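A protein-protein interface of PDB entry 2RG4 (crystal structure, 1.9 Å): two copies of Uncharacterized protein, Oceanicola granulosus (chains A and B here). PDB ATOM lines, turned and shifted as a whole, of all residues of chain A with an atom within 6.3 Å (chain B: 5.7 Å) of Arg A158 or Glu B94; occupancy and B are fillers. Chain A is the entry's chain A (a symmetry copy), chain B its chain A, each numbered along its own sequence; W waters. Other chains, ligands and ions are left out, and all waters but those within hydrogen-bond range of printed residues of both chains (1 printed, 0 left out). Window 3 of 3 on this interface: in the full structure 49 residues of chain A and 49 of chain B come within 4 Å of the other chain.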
ATOM      1  N   PRO A 155       7.505  24.104 -30.479  1.00  0.00           N
ATOM      2  CA  PRO A 155       6.820  25.017 -29.554  1.00  0.00           C
ATOM      3  C   PRO A 155       6.711  26.437 -30.146  1.00  0.00           C
ATOM      4  O   PRO A 155       7.485  26.852 -31.001  1.00  0.00           O
ATOM      5  CB  PRO A 155       7.708  24.998 -28.269  1.00  0.00           C
ATOM      6  CG  PRO A 155       8.795  23.953 -28.464  1.00  0.00           C
ATOM      7  CD  PRO A 155       8.566  23.293 -29.835  1.00  0.00           C
ATOM      8  N   THR A 156       5.675  27.152 -29.741  1.00  0.00           N
ATOM      9  CA  THR A 156       5.575  28.556 -30.066  1.00  0.00           C
ATOM     10  C   THR A 156       6.712  29.252 -29.351  1.00  0.00           C
ATOM     11  O   THR A 156       7.165  28.859 -28.261  1.00  0.00           O
ATOM     12  CB  THR A 156       4.275  29.169 -29.480  1.00  0.00           C
ATOM     13  OG1 THR A 156       4.261  28.890 -28.086  1.00  0.00           O
ATOM     14  CG2 THR A 156       3.039  28.551 -30.111  1.00  0.00           C
ATOM     15  N   ARG A 157       7.084  30.379 -29.891  1.00  0.00           N
ATOM     16  CA  ARG A 157       8.192  31.113 -29.314  1.00  0.00           C
ATOM     17  C   ARG A 157       7.745  32.279 -28.474  1.00  0.00           C
ATOM     18  O   ARG A 157       6.781  32.959 -28.836  1.00  0.00           O
ATOM     19  CB  ARG A 157       8.971  31.693 -30.451  1.00  0.00           C
ATOM     20  CG  ARG A 157       8.777  30.866 -31.662  1.00  0.00           C
ATOM     21  CD  ARG A 157       9.934  29.988 -31.785  1.00  0.00           C
ATOM     22  NE  ARG A 157      10.936  30.843 -32.364  1.00  0.00           N
ATOM     23  CZ  ARG A 157      12.001  30.429 -33.028  1.00  0.00           C
ATOM     24  NH1 ARG A 157      12.788  31.346 -33.537  1.00  0.00           N
ATOM     25  NH2 ARG A 157      12.240  29.131 -33.212  1.00  0.00           N
ATOM     26  N   ARG A 158       8.471  32.534 -27.385  1.00  0.00           N
ATOM     27  CA  ARG A 158       8.272  33.748 -26.539  1.00  0.00           C
ATOM     28  C   ARG A 158       8.425  34.991 -27.408  1.00  0.00           C
ATOM     29  O   ARG A 158       9.218  35.007 -28.374  1.00  0.00           O
ATOM     30  CB  ARG A 158       9.288  33.766 -25.364  1.00  0.00           C
ATOM     31  CG  ARG A 158       9.235  32.554 -24.487  1.00  0.00           C
ATOM     32  CD  ARG A 158      10.489  32.365 -23.575  1.00  0.00           C
ATOM     33  NE  ARG A 158      10.481  31.016 -22.961  1.00  0.00           N
ATOM     34  CZ  ARG A 158       9.643  30.586 -21.995  1.00  0.00           C
ATOM     35  NH1 ARG A 158       8.704  31.393 -21.486  1.00  0.00           N
ATOM     36  NH2 ARG A 158       9.749  29.329 -21.533  1.00  0.00           N
ATOM     37  N   LYS A 159       7.655  36.033 -27.105  1.00  0.00           N
ATOM     38  CA  LYS A 159       7.660  37.270 -27.876  1.00  0.00           C
ATOM     39  C   LYS A 159       8.704  38.127 -27.169  1.00  0.00           C
ATOM     40  O   LYS A 159       8.336  39.059 -26.480  1.00  0.00           O
ATOM     41  CB  LYS A 159       6.285  37.991 -27.822  1.00  0.00           C
ATOM     42  CG  LYS A 159       5.291  37.779 -29.021  1.00  0.00           C
ATOM     43  CD  LYS A 159       5.113  36.324 -29.361  1.00  0.00           C
ATOM     44  CE  LYS A 159       3.833  35.688 -28.760  1.00  0.00           C
ATOM     45  NZ  LYS A 159       4.060  34.183 -28.430  1.00  0.00           N
ATOM     46  N   GLY A 160       9.979  37.748 -27.283  1.00  0.00           N
ATOM     47  CA  GLY A 160      11.076  38.338 -26.487  1.00  0.00           C
ATOM     48  C   GLY A 160      11.733  39.483 -27.235  1.00  0.00           C
ATOM     49  O   GLY A 160      11.235  39.918 -28.269  1.00  0.00           O
ATOM     50  N   LEU A 165      14.544  36.382 -33.555  1.00  0.00           N
ATOM     51  CA  LEU A 165      13.886  35.136 -33.288  1.00  0.00           C
ATOM     52  C   LEU A 165      12.362  35.156 -33.328  1.00  0.00           C
ATOM     53  O   LEU A 165      11.705  34.154 -32.985  1.00  0.00           O
ATOM     54  CB  LEU A 165      14.306  34.609 -31.925  1.00  0.00           C
ATOM     55  CG  LEU A 165      15.790  34.482 -31.755  1.00  0.00           C
ATOM     56  CD1 LEU A 165      16.099  34.519 -30.296  1.00  0.00           C
ATOM     57  CD2 LEU A 165      16.091  33.208 -32.339  1.00  0.00           C
ATOM     58  N   ARG A 166      11.782  36.278 -33.682  1.00  0.00           N
ATOM     59  CA  ARG A 166      10.334  36.425 -33.558  1.00  0.00           C
ATOM     60  C   ARG A 166       9.690  35.916 -34.799  1.00  0.00           C
ATOM     61  O   ARG A 166      10.307  36.021 -35.878  1.00  0.00           O
ATOM     62  CB  ARG A 166       9.959  37.889 -33.442  1.00  0.00           C
ATOM     63  CG  ARG A 166      10.506  38.636 -32.134  1.00  0.00           C
ATOM     64  CD  ARG A 166       9.640  38.196 -30.946  1.00  0.00           C
ATOM     65  NE  ARG A 166       8.324  38.713 -31.212  1.00  0.00           N
ATOM     66  CZ  ARG A 166       7.960  39.950 -30.866  1.00  0.00           C
ATOM     67  NH1 ARG A 166       8.798  40.729 -30.197  1.00  0.00           N
ATOM     68  NH2 ARG A 166       6.762  40.395 -31.146  1.00  0.00           N
ATOM     69  N   GLU B  89      16.238  27.264 -24.804  1.00  0.00           N
ATOM     70  CA  GLU B  89      16.320  28.588 -24.201  1.00  0.00           C
ATOM     71  C   GLU B  89      16.770  29.651 -25.150  1.00  0.00           C
ATOM     72  O   GLU B  89      16.131  30.697 -25.205  1.00  0.00           O
ATOM     73  CB  GLU B  89      17.272  28.645 -23.012  1.00  0.00           C
ATOM     74  CG  GLU B  89      16.613  28.415 -21.708  1.00  0.00           C
ATOM     75  CD  GLU B  89      15.790  29.623 -21.323  1.00  0.00           C
ATOM     76  OE1 GLU B  89      16.412  30.682 -21.070  1.00  0.00           O
ATOM     77  OE2 GLU B  89      14.540  29.497 -21.253  1.00  0.00           O
ATOM     78  N   GLU B  92      14.103  30.395 -27.602  1.00  0.00           N
ATOM     79  CA  GLU B  92      12.954  31.017 -26.959  1.00  0.00           C
ATOM     80  C   GLU B  92      11.686  30.164 -27.002  1.00  0.00           C
ATOM     81  O   GLU B  92      10.574  30.737 -27.007  1.00  0.00           O
ATOM     82  CB  GLU B  92      12.642  32.457 -27.503  1.00  0.00           C
ATOM     83  CG  GLU B  92      13.805  33.493 -27.495  1.00  0.00           C
ATOM     84  CD  GLU B  92      13.916  34.236 -26.207  1.00  0.00           C
ATOM     85  OE1 GLU B  92      13.270  33.808 -25.220  1.00  0.00           O
ATOM     86  OE2 GLU B  92      14.639  35.254 -26.183  1.00  0.00           O
ATOM     87  N   PHE B  93      11.820  28.827 -27.025  1.00  0.00           N
ATOM     88  CA  PHE B  93      10.642  27.967 -26.980  1.00  0.00           C
ATOM     89  C   PHE B  93       9.840  28.177 -25.738  1.00  0.00           C
ATOM     90  O   PHE B  93      10.406  28.351 -24.623  1.00  0.00           O
ATOM     91  CB  PHE B  93      11.036  26.518 -27.013  1.00  0.00           C
ATOM     92  CG  PHE B  93      11.514  26.052 -28.357  1.00  0.00           C
ATOM     93  CD1 PHE B  93      11.092  26.657 -29.498  1.00  0.00           C
ATOM     94  CD2 PHE B  93      12.352  24.955 -28.447  1.00  0.00           C
ATOM     95  CE1 PHE B  93      11.540  26.235 -30.724  1.00  0.00           C
ATOM     96  CE2 PHE B  93      12.790  24.480 -29.664  1.00  0.00           C
ATOM     97  CZ  PHE B  93      12.379  25.133 -30.828  1.00  0.00           C
ATOM     98  N   GLU B  94       8.513  28.176 -25.915  1.00  0.00           N
ATOM     99  CA  GLU B  94       7.589  28.181 -24.784  1.00  0.00           C
ATOM    100  C   GLU B  94       7.239  26.733 -24.541  1.00  0.00           C
ATOM    101  O   GLU B  94       6.493  26.120 -25.298  1.00  0.00           O
ATOM    102  CB  GLU B  94       6.382  29.071 -25.092  1.00  0.00           C
ATOM    103  CG  GLU B  94       5.310  29.185 -23.956  1.00  0.00           C
ATOM    104  CD  GLU B  94       5.886  29.389 -22.524  1.00  0.00           C
ATOM    105  OE1 GLU B  94       6.579  30.426 -22.321  1.00  0.00           O
ATOM    106  OE2 GLU B  94       5.641  28.518 -21.612  1.00  0.00           O
ATOM    107  N   LEU B  95       7.847  26.155 -23.517  1.00  0.00           N
ATOM    108  CA  LEU B  95       7.785  24.714 -23.273  1.00  0.00           C
ATOM    109  C   LEU B  95       6.722  24.287 -22.261  1.00  0.00           C
ATOM    110  O   LEU B  95       6.556  23.064 -22.034  1.00  0.00           O
ATOM    111  CB  LEU B  95       9.120  24.207 -22.739  1.00  0.00           C
ATOM    112  CG  LEU B  95      10.326  24.263 -23.656  1.00  0.00           C
ATOM    113  CD1 LEU B  95      11.554  23.845 -22.874  1.00  0.00           C
ATOM    114  CD2 LEU B  95      10.121  23.388 -24.888  1.00  0.00           C
ATOM    115  N   ASP B  96       6.047  25.270 -21.638  1.00  0.00           N
ATOM    116  CA  ASP B  96       5.206  25.044 -20.424  1.00  0.00           C
ATOM    117  C   ASP B  96       6.050  24.318 -19.378  1.00  0.00           C
ATOM    118  O   ASP B  96       7.210  24.671 -19.158  1.00  0.00           O
ATOM    119  CB  ASP B  96       3.902  24.276 -20.726  1.00  0.00           C
ATOM    120  CG  ASP B  96       3.251  24.705 -22.065  1.00  0.00           C
ATOM    121  OD1 ASP B  96       3.372  25.891 -22.473  1.00  0.00           O
ATOM    122  OD2 ASP B  96       2.615  23.845 -22.726  1.00  0.00           O
ATOM    123  N   TRP B 207       8.848  16.996 -28.036  1.00  0.00           N
ATOM    124  CA  TRP B 207       8.301  17.913 -27.041  1.00  0.00           C
ATOM    125  C   TRP B 207       7.290  17.136 -26.230  1.00  0.00           C
ATOM    126  O   TRP B 207       6.171  17.018 -26.691  1.00  0.00           O
ATOM    127  CB  TRP B 207       7.634  19.111 -27.729  1.00  0.00           C
ATOM    128  CG  TRP B 207       7.196  20.129 -26.778  1.00  0.00           C
ATOM    129  CD1 TRP B 207       7.678  20.343 -25.500  1.00  0.00           C
ATOM    130  CD2 TRP B 207       6.183  21.128 -26.997  1.00  0.00           C
ATOM    131  NE1 TRP B 207       6.997  21.403 -24.914  1.00  0.00           N
ATOM    132  CE2 TRP B 207       6.089  21.905 -25.807  1.00  0.00           C
ATOM    133  CE3 TRP B 207       5.353  21.443 -28.080  1.00  0.00           C
ATOM    134  CZ2 TRP B 207       5.182  22.961 -25.666  1.00  0.00           C
ATOM    135  CZ3 TRP B 207       4.461  22.510 -27.949  1.00  0.00           C
ATOM    136  CH2 TRP B 207       4.367  23.242 -26.744  1.00  0.00           C
HETATM  137  O   HOH W   1       4.158  26.366 -26.731  1.00  0.00           O
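Of the 8 printed residues of chain A, 5 touch a printed residue of chain B. Hydrophobic or aromatic side chains of chain A within 4 Å of the printed part of chain B: Pro A155 and Leu A165. Of the 7 printed residues of chain B, 5 touch a printed residue of chain A. Along chain B the printed residues that touch a printed residue of chain A span positions 92 to 207. Among the printed residues, 12 pairs touch across the chains.
No position is printed for both chains. Of the 12 pairs that touch across the chains among the printed residues, none has its exchanged pair printed and touching as well.
Among the printed residues, pairs that only touch across the chains: Arg A157 with Glu B92 (3.3 Å), Pro A155 with Glu B94 (3.4 Å), Pro A155 with Phe B93 (3.4 Å), Thr A156 with Phe B93 (3.7 Å), Leu A165 with Glu B92 (3.8 Å), Pro A155 with Trp B207 (3.8 Å), Pro A155 with Leu B95 (3.9 Å) and Arg A157 with Phe B93 (3.9 Å).
The backbone carbonyl oxygen of Glu B92 lies within hydrogen-bond range of the backbone NH of Arg A158 (2.8 Å). The guanidinium group of Arg A158 sits at hydrogen-bond distance from the backbone carbonyl oxygen of Phe B93, at 3.1 Å. O of Thr A156 sits at hydrogen-bond distance from N of Glu B94, at 2.8 Å. The side-chain carboxylate (OE1) of Glu B94 is in salt-bridge range of the guanidinium group (NH1) of Arg A158 (2.5 Å).
The side-chain carboxylate (OE2) of Glu B94 is in hydrogen-bond range of the backbone NH (N) of Asp B96. The backbone carbonyl oxygen of Leu B95 lies within hydrogen-bond range of the indole nitrogen of Trp B207, at 3.4 Å. The backbone carbonyl oxygen of Arg A157 lies within hydrogen-bond range of the side-chain amino group of Lys A159 (3.0 Å). O of Leu A165 sits at hydrogen-bond distance from NH1 of Arg A157, 3.1 Å away.
Water W1 bridges O of Glu B94 (2.8 Å) and OG1 of Thr A156 (2.9 Å).
Of the printed residues of chain B, Thr A156 touches Phe B93 and Glu B94. Arg A158 touches just these residues of chain B: Glu B92, Phe B93 and Glu B94. Printed residues of chain A within 4 Å of Glu B92: Arg A157, Arg A158 and Leu A165. Printed residues of chain A within 4 Å of Phe B93: Pro A155 (3.4 Å), Thr A156 (3.7 Å), Arg A157 (3.9 Å) and Arg A158 (3.1 Å). The nearest printed residue of chain A that does not touch Leu B95 is Arg A158 (4.2 Å).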
